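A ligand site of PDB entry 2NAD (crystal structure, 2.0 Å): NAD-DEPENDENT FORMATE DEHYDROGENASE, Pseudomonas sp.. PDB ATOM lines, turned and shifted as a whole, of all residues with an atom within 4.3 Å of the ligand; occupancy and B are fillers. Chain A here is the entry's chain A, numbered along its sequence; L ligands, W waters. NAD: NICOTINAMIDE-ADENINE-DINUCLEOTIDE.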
ATOM      1  N   PHE A  98      -6.007  -9.528 -14.464  1.00  0.00           N
ATOM      2  CA  PHE A  98      -6.929  -9.270 -15.564  1.00  0.00           C
ATOM      3  C   PHE A  98      -8.253  -9.961 -15.374  1.00  0.00           C
ATOM      4  O   PHE A  98      -9.209  -9.512 -15.992  1.00  0.00           O
ATOM      5  CB  PHE A  98      -6.292  -9.713 -16.886  1.00  0.00           C
ATOM      6  CG  PHE A  98      -4.799  -9.664 -16.789  1.00  0.00           C
ATOM      7  CD1 PHE A  98      -4.212  -8.423 -16.777  1.00  0.00           C
ATOM      8  CD2 PHE A  98      -4.007 -10.768 -16.657  1.00  0.00           C
ATOM      9  CE1 PHE A  98      -2.835  -8.237 -16.658  1.00  0.00           C
ATOM     10  CE2 PHE A  98      -2.663 -10.584 -16.470  1.00  0.00           C
ATOM     11  CZ  PHE A  98      -2.060  -9.355 -16.482  1.00  0.00           C
ATOM     12  N   ILE A 122       1.331  -8.914 -11.911  1.00  0.00           N
ATOM     13  CA  ILE A 122       1.830  -8.012 -10.892  1.00  0.00           C
ATOM     14  C   ILE A 122       0.657  -7.249 -10.319  1.00  0.00           C
ATOM     15  O   ILE A 122      -0.231  -6.831 -11.059  1.00  0.00           O
ATOM     16  CB  ILE A 122       2.817  -7.004 -11.521  1.00  0.00           C
ATOM     17  CG1 ILE A 122       4.148  -7.685 -11.864  1.00  0.00           C
ATOM     18  CG2 ILE A 122       3.109  -5.825 -10.615  1.00  0.00           C
ATOM     19  CD1 ILE A 122       4.884  -6.732 -12.829  1.00  0.00           C
ATOM     20  N   GLY A 123       0.663  -7.104  -9.005  1.00  0.00           N
ATOM     21  CA  GLY A 123      -0.377  -6.341  -8.343  1.00  0.00           C
ATOM     22  C   GLY A 123      -1.224  -7.285  -7.562  1.00  0.00           C
ATOM     23  O   GLY A 123      -2.030  -7.923  -8.195  1.00  0.00           O
ATOM     24  N   ASP A 125      -3.390  -6.574  -4.946  1.00  0.00           N
ATOM     25  CA  ASP A 125      -4.453  -5.826  -4.269  1.00  0.00           C
ATOM     26  C   ASP A 125      -5.815  -6.461  -4.239  1.00  0.00           C
ATOM     27  O   ASP A 125      -6.751  -6.101  -3.539  1.00  0.00           O
ATOM     28  CB  ASP A 125      -4.488  -4.407  -4.848  1.00  0.00           C
ATOM     29  CG  ASP A 125      -4.518  -4.554  -6.381  1.00  0.00           C
ATOM     30  OD1 ASP A 125      -3.506  -4.631  -7.074  1.00  0.00           O
ATOM     31  OD2 ASP A 125      -5.661  -4.643  -6.857  1.00  0.00           O
ATOM     32  N   ASN A 146       5.648  -7.953 -16.537  1.00  0.00           N
ATOM     33  CA  ASN A 146       4.986  -7.086 -17.513  1.00  0.00           C
ATOM     34  C   ASN A 146       5.183  -5.620 -17.220  1.00  0.00           C
ATOM     35  O   ASN A 146       4.409  -4.866 -17.790  1.00  0.00           O
ATOM     36  CB  ASN A 146       3.524  -7.511 -17.652  1.00  0.00           C
ATOM     37  CG  ASN A 146       2.758  -7.424 -16.353  1.00  0.00           C
ATOM     38  OD1 ASN A 146       3.179  -6.636 -15.537  1.00  0.00           O
ATOM     39  ND2 ASN A 146       1.707  -8.192 -16.188  1.00  0.00           N
ATOM     40  N   SER A 147       6.119  -5.159 -16.406  1.00  0.00           N
ATOM     41  CA  SER A 147       6.329  -3.726 -16.205  1.00  0.00           C
ATOM     42  C   SER A 147       6.656  -3.010 -17.507  1.00  0.00           C
ATOM     43  O   SER A 147       6.179  -1.914 -17.747  1.00  0.00           O
ATOM     44  CB  SER A 147       7.526  -3.520 -15.248  1.00  0.00           C
ATOM     45  OG  SER A 147       7.117  -4.175 -14.068  1.00  0.00           O
ATOM     46  N   VAL A 150       3.370  -2.764 -19.768  1.00  0.00           N
ATOM     47  CA  VAL A 150       2.541  -1.713 -19.257  1.00  0.00           C
ATOM     48  C   VAL A 150       3.089  -0.320 -19.595  1.00  0.00           C
ATOM     49  O   VAL A 150       2.325   0.539 -19.971  1.00  0.00           O
ATOM     50  CB  VAL A 150       2.334  -1.823 -17.754  1.00  0.00           C
ATOM     51  CG1 VAL A 150       1.456  -0.681 -17.281  1.00  0.00           C
ATOM     52  CG2 VAL A 150       1.729  -3.163 -17.337  1.00  0.00           C
ATOM     53  N   VAL A 197       2.992   9.426 -11.001  1.00  0.00           N
ATOM     54  CA  VAL A 197       2.898   9.213  -9.532  1.00  0.00           C
ATOM     55  C   VAL A 197       3.605   7.857  -9.408  1.00  0.00           C
ATOM     56  O   VAL A 197       3.019   6.840  -9.914  1.00  0.00           O
ATOM     57  CB  VAL A 197       1.500   9.009  -8.994  1.00  0.00           C
ATOM     58  CG1 VAL A 197       1.578   8.610  -7.514  1.00  0.00           C
ATOM     59  CG2 VAL A 197       0.730  10.303  -9.204  1.00  0.00           C
ATOM     60  N   ALA A 198       4.770   7.762  -8.853  1.00  0.00           N
ATOM     61  CA  ALA A 198       5.631   6.630  -8.672  1.00  0.00           C
ATOM     62  C   ALA A 198       6.522   6.392  -9.891  1.00  0.00           C
ATOM     63  O   ALA A 198       6.188   6.502 -11.100  1.00  0.00           O
ATOM     64  CB  ALA A 198       4.991   5.315  -8.281  1.00  0.00           C
ATOM     65  N   ALA A 199       7.739   6.042  -9.563  1.00  0.00           N
ATOM     66  CA  ALA A 199       8.826   5.748 -10.427  1.00  0.00           C
ATOM     67  C   ALA A 199       9.484   4.440 -10.043  1.00  0.00           C
ATOM     68  O   ALA A 199      10.658   4.310  -9.824  1.00  0.00           O
ATOM     69  CB  ALA A 199       9.845   6.837 -10.619  1.00  0.00           C
ATOM     70  N   GLY A 200       8.672   3.409 -10.068  1.00  0.00           N
ATOM     71  CA  GLY A 200       9.134   2.061  -9.848  1.00  0.00           C
ATOM     72  C   GLY A 200       9.497   1.494 -11.223  1.00  0.00           C
ATOM     73  O   GLY A 200       9.870   2.172 -12.174  1.00  0.00           O
ATOM     74  N   ARG A 201       9.330   0.184 -11.348  1.00  0.00           N
ATOM     75  CA  ARG A 201       9.654  -0.528 -12.583  1.00  0.00           C
ATOM     76  C   ARG A 201       8.840   0.052 -13.746  1.00  0.00           C
ATOM     77  O   ARG A 201       9.492   0.366 -14.754  1.00  0.00           O
ATOM     78  CB  ARG A 201       9.476  -2.035 -12.387  1.00  0.00           C
ATOM     79  CG  ARG A 201      10.475  -2.539 -11.376  1.00  0.00           C
ATOM     80  CD  ARG A 201      10.099  -3.971 -11.057  1.00  0.00           C
ATOM     81  NE  ARG A 201      11.056  -4.524 -10.107  1.00  0.00           N
ATOM     82  CZ  ARG A 201      10.906  -4.402  -8.782  1.00  0.00           C
ATOM     83  NH1 ARG A 201       9.913  -3.826  -8.107  1.00  0.00           N
ATOM     84  NH2 ARG A 201      11.876  -4.971  -8.037  1.00  0.00           N
ATOM     85  N   ILE A 202       7.549   0.250 -13.621  1.00  0.00           N
ATOM     86  CA  ILE A 202       6.797   0.809 -14.743  1.00  0.00           C
ATOM     87  C   ILE A 202       7.080   2.291 -14.936  1.00  0.00           C
ATOM     88  O   ILE A 202       7.303   2.741 -16.038  1.00  0.00           O
ATOM     89  CB  ILE A 202       5.273   0.662 -14.573  1.00  0.00           C
ATOM     90  CG1 ILE A 202       4.920  -0.825 -14.478  1.00  0.00           C
ATOM     91  CG2 ILE A 202       4.445   1.371 -15.619  1.00  0.00           C
ATOM     92  CD1 ILE A 202       3.591  -1.334 -14.136  1.00  0.00           C
ATOM     93  N   ASP A 221       7.380   9.812  -5.623  1.00  0.00           N
ATOM     94  CA  ASP A 221       7.410   8.424  -5.239  1.00  0.00           C
ATOM     95  C   ASP A 221       7.710   8.334  -3.739  1.00  0.00           C
ATOM     96  O   ASP A 221       8.269   9.268  -3.172  1.00  0.00           O
ATOM     97  CB  ASP A 221       8.501   7.636  -5.918  1.00  0.00           C
ATOM     98  CG  ASP A 221       8.351   6.165  -5.811  1.00  0.00           C
ATOM     99  OD1 ASP A 221       8.385   5.576  -4.718  1.00  0.00           O
ATOM    100  OD2 ASP A 221       8.265   5.451  -6.838  1.00  0.00           O
ATOM    101  N   ARG A 222       7.345   7.256  -3.110  1.00  0.00           N
ATOM    102  CA  ARG A 222       7.633   7.039  -1.670  1.00  0.00           C
ATOM    103  C   ARG A 222       9.165   6.955  -1.541  1.00  0.00           C
ATOM    104  O   ARG A 222       9.677   7.415  -0.515  1.00  0.00           O
ATOM    105  CB  ARG A 222       6.973   5.744  -1.196  1.00  0.00           C
ATOM    106  CG  ARG A 222       7.372   5.043   0.062  1.00  0.00           C
ATOM    107  CD  ARG A 222       6.932   3.603   0.190  1.00  0.00           C
ATOM    108  NE  ARG A 222       5.612   3.266   0.610  1.00  0.00           N
ATOM    109  CZ  ARG A 222       5.082   2.089   0.982  1.00  0.00           C
ATOM    110  NH1 ARG A 222       5.774   0.959   1.031  1.00  0.00           N
ATOM    111  NH2 ARG A 222       3.799   2.122   1.339  1.00  0.00           N
ATOM    112  N   HIS A 223       9.828   6.365  -2.552  1.00  0.00           N
ATOM    113  CA  HIS A 223      11.264   6.224  -2.574  1.00  0.00           C
ATOM    114  C   HIS A 223      11.827   7.058  -3.734  1.00  0.00           C
ATOM    115  O   HIS A 223      11.570   6.854  -4.916  1.00  0.00           O
ATOM    116  CB  HIS A 223      11.655   4.757  -2.802  1.00  0.00           C
ATOM    117  CG  HIS A 223      11.086   3.855  -1.770  1.00  0.00           C
ATOM    118  ND1 HIS A 223      11.591   3.855  -0.456  1.00  0.00           N
ATOM    119  CD2 HIS A 223      10.083   2.936  -1.797  1.00  0.00           C
ATOM    120  CE1 HIS A 223      10.904   2.963   0.261  1.00  0.00           C
ATOM    121  NE2 HIS A 223      10.011   2.397  -0.524  1.00  0.00           N
ATOM    122  N   ASN A 254       1.291   5.247 -11.667  1.00  0.00           N
ATOM    123  CA  ASN A 254       2.045   4.018 -11.704  1.00  0.00           C
ATOM    124  C   ASN A 254       2.406   3.420 -10.354  1.00  0.00           C
ATOM    125  O   ASN A 254       3.353   2.679 -10.225  1.00  0.00           O
ATOM    126  CB  ASN A 254       3.263   4.253 -12.598  1.00  0.00           C
ATOM    127  CG  ASN A 254       2.913   4.441 -14.074  1.00  0.00           C
ATOM    128  OD1 ASN A 254       2.410   3.565 -14.758  1.00  0.00           O
ATOM    129  ND2 ASN A 254       3.123   5.678 -14.462  1.00  0.00           N
ATOM    130  N   CYS A 255       1.597   3.692  -9.377  1.00  0.00           N
ATOM    131  CA  CYS A 255       1.768   3.134  -8.025  1.00  0.00           C
ATOM    132  C   CYS A 255       0.750   1.983  -7.800  1.00  0.00           C
ATOM    133  O   CYS A 255      -0.280   1.823  -8.434  1.00  0.00           O
ATOM    134  CB  CYS A 255       1.545   4.229  -6.967  1.00  0.00           C
ATOM    135  SG  CYS A 255      -0.057   5.013  -7.212  1.00  0.00           S
ATOM    136  N   PRO A 256       1.071   1.194  -6.766  1.00  0.00           N
ATOM    137  CA  PRO A 256       0.233   0.059  -6.361  1.00  0.00           C
ATOM    138  C   PRO A 256      -0.986   0.610  -5.612  1.00  0.00           C
ATOM    139  O   PRO A 256      -0.932   1.762  -5.169  1.00  0.00           O
ATOM    140  CB  PRO A 256       1.083  -0.856  -5.468  1.00  0.00           C
ATOM    141  CG  PRO A 256       2.427  -0.153  -5.428  1.00  0.00           C
ATOM    142  CD  PRO A 256       2.270   1.275  -5.913  1.00  0.00           C
ATOM    143  N   HIS A 258      -3.155   0.569  -2.444  1.00  0.00           N
ATOM    144  CA  HIS A 258      -3.095   0.173  -1.032  1.00  0.00           C
ATOM    145  C   HIS A 258      -3.768   1.361  -0.397  1.00  0.00           C
ATOM    146  O   HIS A 258      -4.119   2.395  -0.982  1.00  0.00           O
ATOM    147  CB  HIS A 258      -1.721  -0.340  -0.631  1.00  0.00           C
ATOM    148  CG  HIS A 258      -0.594   0.600  -0.750  1.00  0.00           C
ATOM    149  ND1 HIS A 258      -0.471   1.718   0.048  1.00  0.00           N
ATOM    150  CD2 HIS A 258       0.430   0.627  -1.615  1.00  0.00           C
ATOM    151  CE1 HIS A 258       0.631   2.351  -0.311  1.00  0.00           C
ATOM    152  NE2 HIS A 258       1.215   1.732  -1.325  1.00  0.00           N
ATOM    153  N   GLU A 260      -2.707   3.841   1.217  1.00  0.00           N
ATOM    154  CA  GLU A 260      -2.250   5.189   0.990  1.00  0.00           C
ATOM    155  C   GLU A 260      -2.623   5.698  -0.412  1.00  0.00           C
ATOM    156  O   GLU A 260      -2.597   6.926  -0.551  1.00  0.00           O
ATOM    157  CB  GLU A 260      -0.735   5.254   1.072  1.00  0.00           C
ATOM    158  CG  GLU A 260      -0.136   4.880   2.413  1.00  0.00           C
ATOM    159  CD  GLU A 260       1.391   4.826   2.398  1.00  0.00           C
ATOM    160  OE1 GLU A 260       2.081   4.853   1.331  1.00  0.00           O
ATOM    161  OE2 GLU A 260       1.806   4.736   3.591  1.00  0.00           O
ATOM    162  N   THR A 261      -2.952   4.886  -1.387  1.00  0.00           N
ATOM    163  CA  THR A 261      -3.227   5.397  -2.737  1.00  0.00           C
ATOM    164  C   THR A 261      -4.660   5.253  -3.185  1.00  0.00           C
ATOM    165  O   THR A 261      -5.115   5.825  -4.168  1.00  0.00           O
ATOM    166  CB  THR A 261      -2.263   4.608  -3.647  1.00  0.00           C
ATOM    167  OG1 THR A 261      -2.538   3.184  -3.510  1.00  0.00           O
ATOM    168  CG2 THR A 261      -0.830   4.903  -3.280  1.00  0.00           C
ATOM    169  N   THR A 282      -3.021   2.898 -15.847  1.00  0.00           N
ATOM    170  CA  THR A 282      -2.837   1.498 -16.123  1.00  0.00           C
ATOM    171  C   THR A 282      -2.378   0.872 -14.810  1.00  0.00           C
ATOM    172  O   THR A 282      -1.865  -0.217 -14.872  1.00  0.00           O
ATOM    173  CB  THR A 282      -1.735   1.249 -17.166  1.00  0.00           C
ATOM    174  OG1 THR A 282      -0.574   1.894 -16.640  1.00  0.00           O
ATOM    175  CG2 THR A 282      -2.118   1.844 -18.511  1.00  0.00           C
ATOM    176  N   ALA A 283      -2.473   1.453 -13.628  1.00  0.00           N
ATOM    177  CA  ALA A 283      -2.055   0.910 -12.344  1.00  0.00           C
ATOM    178  C   ALA A 283      -3.200   0.089 -11.781  1.00  0.00           C
ATOM    179  O   ALA A 283      -3.239  -1.144 -11.925  1.00  0.00           O
ATOM    180  CB  ALA A 283      -1.588   1.987 -11.372  1.00  0.00           C
ATOM    181  N   ARG A 284      -4.177   0.753 -11.145  1.00  0.00           N
ATOM    182  CA  ARG A 284      -5.381   0.135 -10.595  1.00  0.00           C
ATOM    183  C   ARG A 284      -6.558   1.116 -10.667  1.00  0.00           C
ATOM    184  O   ARG A 284      -6.460   2.338 -10.462  1.00  0.00           O
ATOM    185  CB  ARG A 284      -5.152  -0.435  -9.192  1.00  0.00           C
ATOM    186  CG  ARG A 284      -4.316  -1.694  -9.018  1.00  0.00           C
ATOM    187  CD  ARG A 284      -5.001  -2.874  -9.749  1.00  0.00           C
ATOM    188  NE  ARG A 284      -4.217  -4.095  -9.577  1.00  0.00           N
ATOM    189  CZ  ARG A 284      -3.405  -4.587 -10.510  1.00  0.00           C
ATOM    190  NH1 ARG A 284      -3.190  -3.991 -11.691  1.00  0.00           N
ATOM    191  NH2 ARG A 284      -2.804  -5.742 -10.288  1.00  0.00           N
ATOM    192  N   ASP A 308      -6.484   0.773 -18.700  1.00  0.00           N
ATOM    193  CA  ASP A 308      -6.928  -0.586 -18.933  1.00  0.00           C
ATOM    194  C   ASP A 308      -7.446  -1.227 -17.642  1.00  0.00           C
ATOM    195  O   ASP A 308      -8.019  -2.325 -17.645  1.00  0.00           O
ATOM    196  CB  ASP A 308      -5.808  -1.393 -19.596  1.00  0.00           C
ATOM    197  CG  ASP A 308      -4.626  -1.617 -18.720  1.00  0.00           C
ATOM    198  OD1 ASP A 308      -4.317  -0.852 -17.810  1.00  0.00           O
ATOM    199  OD2 ASP A 308      -3.942  -2.615 -18.952  1.00  0.00           O
ATOM    200  N   VAL A 309      -7.341  -0.529 -16.527  1.00  0.00           N
ATOM    201  CA  VAL A 309      -7.749  -1.008 -15.236  1.00  0.00           C
ATOM    202  C   VAL A 309      -8.987  -0.350 -14.674  1.00  0.00           C
ATOM    203  O   VAL A 309      -9.310   0.822 -14.826  1.00  0.00           O
ATOM    204  CB  VAL A 309      -6.553  -0.950 -14.249  1.00  0.00           C
ATOM    205  CG1 VAL A 309      -5.408  -1.828 -14.647  1.00  0.00           C
ATOM    206  CG2 VAL A 309      -6.085   0.485 -14.168  1.00  0.00           C
ATOM    207  N   HIS A 332      -8.659  -4.868 -19.241  1.00  0.00           N
ATOM    208  CA  HIS A 332      -7.374  -5.102 -18.648  1.00  0.00           C
ATOM    209  C   HIS A 332      -6.523  -6.140 -19.347  1.00  0.00           C
ATOM    210  O   HIS A 332      -6.526  -7.345 -19.143  1.00  0.00           O
ATOM    211  CB  HIS A 332      -7.610  -5.509 -17.200  1.00  0.00           C
ATOM    212  CG  HIS A 332      -6.358  -5.387 -16.422  1.00  0.00           C
ATOM    213  ND1 HIS A 332      -6.274  -5.821 -15.124  1.00  0.00           N
ATOM    214  CD2 HIS A 332      -5.140  -4.908 -16.741  1.00  0.00           C
ATOM    215  CE1 HIS A 332      -5.038  -5.580 -14.696  1.00  0.00           C
ATOM    216  NE2 HIS A 332      -4.343  -5.021 -15.637  1.00  0.00           N
ATOM    217  N   SER A 334      -2.908  -4.864 -20.858  1.00  0.00           N
ATOM    218  CA  SER A 334      -1.562  -4.427 -21.024  1.00  0.00           C
ATOM    219  C   SER A 334      -0.594  -5.491 -20.551  1.00  0.00           C
ATOM    220  O   SER A 334       0.349  -5.783 -21.277  1.00  0.00           O
ATOM    221  CB  SER A 334      -1.230  -3.043 -20.446  1.00  0.00           C
ATOM    222  OG  SER A 334      -1.494  -3.040 -19.062  1.00  0.00           O
ATOM    223  N   GLY A 335      -0.815  -6.029 -19.383  1.00  0.00           N
ATOM    224  CA  GLY A 335       0.069  -7.021 -18.838  1.00  0.00           C
ATOM    225  C   GLY A 335      -0.095  -8.482 -19.249  1.00  0.00           C
ATOM    226  O   GLY A 335       0.568  -9.379 -18.781  1.00  0.00           O
ATOM    227  N   THR A 376       9.357  -7.317  -1.836  1.00  0.00           N
ATOM    228  CA  THR A 376       8.760  -6.190  -2.556  1.00  0.00           C
ATOM    229  C   THR A 376       7.566  -5.557  -1.878  1.00  0.00           C
ATOM    230  O   THR A 376       7.305  -4.343  -2.013  1.00  0.00           O
ATOM    231  CB  THR A 376       8.530  -6.636  -4.032  1.00  0.00           C
ATOM    232  OG1 THR A 376       9.812  -6.896  -4.650  1.00  0.00           O
ATOM    233  CG2 THR A 376       7.747  -5.595  -4.844  1.00  0.00           C
ATOM    234  N   HIS A 379       8.630  -2.889   0.476  1.00  0.00           N
ATOM    235  CA  HIS A 379       9.100  -1.815  -0.305  1.00  0.00           C
ATOM    236  C   HIS A 379       7.947  -1.004  -0.890  1.00  0.00           C
ATOM    237  O   HIS A 379       7.938   0.224  -0.808  1.00  0.00           O
ATOM    238  CB  HIS A 379       9.921  -2.281  -1.547  1.00  0.00           C
ATOM    239  CG  HIS A 379      10.694  -1.152  -2.195  1.00  0.00           C
ATOM    240  ND1 HIS A 379      10.334  -0.608  -3.439  1.00  0.00           N
ATOM    241  CD2 HIS A 379      11.791  -0.458  -1.803  1.00  0.00           C
ATOM    242  CE1 HIS A 379      11.195   0.354  -3.734  1.00  0.00           C
ATOM    243  NE2 HIS A 379      12.085   0.483  -2.777  1.00  0.00           N
ATOM    244  N   SER A 380       7.037  -1.650  -1.565  1.00  0.00           N
ATOM    245  CA  SER A 380       6.002  -0.886  -2.270  1.00  0.00           C
ATOM    246  C   SER A 380       4.609  -0.797  -1.682  1.00  0.00           C
ATOM    247  O   SER A 380       3.763  -0.025  -2.188  1.00  0.00           O
ATOM    248  CB  SER A 380       5.967  -1.479  -3.722  1.00  0.00           C
ATOM    249  OG  SER A 380       7.221  -1.392  -4.378  1.00  0.00           O
ATOM    250  N   TYR A 381       4.318  -1.605  -0.666  1.00  0.00           N
ATOM    251  CA  TYR A 381       2.977  -1.588  -0.123  1.00  0.00           C
ATOM    252  C   TYR A 381       3.022  -1.097   1.334  1.00  0.00           C
ATOM    253  O   TYR A 381       4.011  -0.834   1.999  1.00  0.00           O
ATOM    254  CB  TYR A 381       2.436  -3.047  -0.220  1.00  0.00           C
ATOM    255  CG  TYR A 381       1.994  -3.525  -1.583  1.00  0.00           C
ATOM    256  CD1 TYR A 381       2.890  -3.906  -2.570  1.00  0.00           C
ATOM    257  CD2 TYR A 381       0.626  -3.606  -1.936  1.00  0.00           C
ATOM    258  CE1 TYR A 381       2.475  -4.298  -3.822  1.00  0.00           C
ATOM    259  CE2 TYR A 381       0.189  -4.024  -3.203  1.00  0.00           C
ATOM    260  CZ  TYR A 381       1.150  -4.376  -4.142  1.00  0.00           C
ATOM    261  OH  TYR A 381       0.753  -4.793  -5.396  1.00  0.00           O
HETATM  262  PA  NAD L   1       7.098  -1.503  -8.394  1.00  0.00           P
HETATM  263  O1A NAD L   1       6.866  -2.074  -6.998  1.00  0.00           O
HETATM  264  O2A NAD L   1       8.361  -1.661  -9.107  1.00  0.00           O
HETATM  265  O5B NAD L   1       6.642   0.000  -8.493  1.00  0.00           O
HETATM  266  C5B NAD L   1       5.798   0.596  -7.439  1.00  0.00           C
HETATM  267  C4B NAD L   1       6.385   1.940  -7.119  1.00  0.00           C
HETATM  268  O4B NAD L   1       5.297   2.605  -6.371  1.00  0.00           O
HETATM  269  C3B NAD L   1       7.554   1.853  -6.045  1.00  0.00           C
HETATM  270  O3B NAD L   1       8.549   2.799  -6.559  1.00  0.00           O
HETATM  271  C2B NAD L   1       6.958   2.374  -4.737  1.00  0.00           C
HETATM  272  O2B NAD L   1       7.784   3.088  -3.949  1.00  0.00           O
HETATM  273  C1B NAD L   1       5.901   3.300  -5.368  1.00  0.00           C
HETATM  274  N9A NAD L   1       4.932   3.680  -4.378  1.00  0.00           N
HETATM  275  C8A NAD L   1       4.377   2.923  -3.378  1.00  0.00           C
HETATM  276  N7A NAD L   1       3.503   3.540  -2.605  1.00  0.00           N
HETATM  277  C5A NAD L   1       3.441   4.788  -3.065  1.00  0.00           C
HETATM  278  C6A NAD L   1       2.710   5.941  -2.518  1.00  0.00           C
HETATM  279  N6A NAD L   1       1.920   5.858  -1.459  1.00  0.00           N
HETATM  280  N1A NAD L   1       2.921   7.055  -3.275  1.00  0.00           N
HETATM  281  C2A NAD L   1       3.696   7.167  -4.364  1.00  0.00           C
HETATM  282  N3A NAD L   1       4.492   6.116  -4.858  1.00  0.00           N
HETATM  283  C4A NAD L   1       4.309   4.917  -4.183  1.00  0.00           C
HETATM  284  O3  NAD L   1       5.975  -2.138  -9.254  1.00  0.00           O
HETATM  285  PN  NAD L   1       5.671  -1.922 -10.874  1.00  0.00           P
HETATM  286  O1N NAD L   1       6.116  -0.568 -11.130  1.00  0.00           O
HETATM  287  O2N NAD L   1       6.160  -3.084 -11.630  1.00  0.00           O
HETATM  288  O5D NAD L   1       4.072  -1.944 -10.811  1.00  0.00           O
HETATM  289  C5D NAD L   1       3.259  -0.889 -10.160  1.00  0.00           C
HETATM  290  C4D NAD L   1       1.848  -1.247 -10.038  1.00  0.00           C
HETATM  291  O4D NAD L   1       1.267  -1.186 -11.443  1.00  0.00           O
HETATM  292  C3D NAD L   1       1.507  -2.764  -9.719  1.00  0.00           C
HETATM  293  O3D NAD L   1       1.448  -2.757  -8.292  1.00  0.00           O
HETATM  294  C2D NAD L   1       0.071  -2.917 -10.258  1.00  0.00           C
HETATM  295  O2D NAD L   1      -0.895  -2.341  -9.465  1.00  0.00           O
HETATM  296  C1D NAD L   1       0.155  -2.039 -11.576  1.00  0.00           C
HETATM  297  N1N NAD L   1       0.298  -2.962 -12.784  1.00  0.00           N
HETATM  298  C2N NAD L   1      -0.743  -2.928 -13.735  1.00  0.00           C
HETATM  299  C3N NAD L   1      -0.542  -3.835 -14.751  1.00  0.00           C
HETATM  300  C7N NAD L   1      -1.555  -3.789 -15.973  1.00  0.00           C
HETATM  301  O7N NAD L   1      -1.345  -4.883 -16.600  1.00  0.00           O
HETATM  302  N7N NAD L   1      -2.294  -2.663 -16.289  1.00  0.00           N
HETATM  303  C4N NAD L   1       0.533  -4.774 -14.937  1.00  0.00           C
HETATM  304  C5N NAD L   1       1.483  -4.681 -13.887  1.00  0.00           C
HETATM  305  C6N NAD L   1       1.338  -3.800 -12.818  1.00  0.00           C
HETATM  306  O   HOH W   1      -1.452  -2.919  -6.602  1.00  0.00           O
HETATM  307  O   HOH W   2      11.136   1.899  -6.060  1.00  0.00           O
HETATM  308  O   HOH W   3       1.554   8.879  -0.127  1.00  0.00           O
HETATM  309  O   HOH W   4       6.963  -5.479 -10.700  1.00  0.00           O
HETATM  310  O   HOH W   5       2.776  -4.980  -7.042  1.00  0.00           O
HETATM  311  O   HOH W   6       6.160   2.259 -10.972  1.00  0.00           O
HETATM  312  O   HOH W   7       1.989   9.553  -3.546  1.00  0.00           O
HETATM  313  O   HOH W   8      10.703  -0.432  -7.413  1.00  0.00           O
HETATM  314  O   HOH W   9       5.311  -4.214  -6.555  1.00  0.00           O
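OE1 of Glu 260 is in hydrogen-bond range of N6A of the ligand, at 3.0 Å.
N of Ile 202 lies within hydrogen-bond range of O1N of the ligand, at 3.0 Å.
A ring nitrogen (NE2) of His 258 sits at hydrogen-bond distance from a nitrogen (N7A) of the ligand, 3.2 Å away.
N of Gly 335 lies within hydrogen-bond range of O7N of the ligand, at 3.1 Å.
The backbone carbonyl oxygen (O) of Thr 282 lies within hydrogen-bond range of a nitrogen (N7N) of the ligand, at 2.9 Å.
OG of Ser 334 is in hydrogen-bond range of N7N of the ligand (2.9 Å).
The side-chain carboxylate (OD1) of Asp 221 is in hydrogen-bond range of an oxygen (O2B) of the ligand (2.7 Å).
N of Arg 201 lies within hydrogen-bond range of O2A of the ligand (3.1 Å).
The side-chain hydroxyl (OG) of Ser 380 sits at hydrogen-bond distance from an oxygen (O1A) of the ligand (2.7 Å).
The guanidinium group of Arg 201 is in salt-bridge range of an oxygen (O2A) of the ligand (2.8 Å).
An oxygen (O2N) of the ligand sits at hydrogen-bond distance from the side-chain hydroxyl (OG) of Ser 147, at 2.8 Å.
An oxygen (O7N) of the ligand sits close to a ring nitrogen (NE2) of His 332.
N7N of the ligand lies within hydrogen-bond range of OD1 of Asp 308.
N of His 223 is in hydrogen-bond range of OD1 of Asp 221, 2.7 Å away.
The side-chain hydroxyl of Ser 334 sits at hydrogen-bond distance from the side-chain carboxylate of Asp 308 (2.5 Å).
The guanidinium group of Arg 284 is in salt-bridge range of the side-chain carboxylate of Asp 125 (2.7 Å).
N of His 258 lies within hydrogen-bond range of OG1 of Thr 261, at 2.9 Å.
NH1 of Arg 222 is in hydrogen-bond range of O of His 379, 2.9 Å away.
The backbone carbonyl oxygen of Tyr 381 lies within hydrogen-bond range of the guanidinium group of Arg 222, at 2.7 Å.
The backbone NH of Glu 260 sits close to a ring nitrogen (ND1) of His 258 (3.3 Å).
O of Val 197 sits at hydrogen-bond distance from N of Asn 254 (2.9 Å).
Phe 98 touches the ligand (CE1 to O7N, 3.7 Å).
Ile 122 touches the ligand.
CA of Gly 123 touches C2D of the ligand (3.9 Å).
Asn 146 touches the ligand (OD1 to C5N, 3.1 Å).
Val 150 touches the ligand.
Ala 198 touches the ligand (CB to O4B, 3.3 Å).
Ala 199 touches the ligand.
CA of Gly 200 touches O3B of the ligand, 3.4 Å away.
Arg 222 touches the ligand (N to N3A, 3.5 Å).
His 223 touches the ligand (CD2 to O2B, 3.2 Å).
Asn 254 touches the ligand.
Cys 255 touches the ligand.
CD of Pro 256 touches O4B of the ligand (3.3 Å).
Thr 261 touches the ligand.
Ala 283 touches the ligand.
Arg 284 touches the ligand.
Val 309 touches the ligand (CG1 to N7N, 3.6 Å).
OH of Tyr 381 touches O3D of the ligand, at 3.6 Å.
Hydrophobic or aromatic side chains that line the ligand: Phe 98, Ile 122, Val 150, Ala 198, Ile 202, His 223, Pro 256, His 258, Val 309 and His 332.
The nearest printed residue that does not touch the ligand is Val 197 (4.1 Å).
Water W6 lies within hydrogen-bond range of O1N of the ligand, N of Gly 200 and O of Asn 254.
Water W5 bridges the side-chain hydroxyl (OH) of Tyr 381 (2.6 Å) and an oxygen (O3D) of the ligand (2.9 Å).
Water W1 lies within hydrogen-bond range of the side-chain carboxylate of Asp 125 (2.7 Å), an oxygen (O2D) of the ligand (3.0 Å) and the side-chain hydroxyl of Tyr 381 (3.1 Å).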
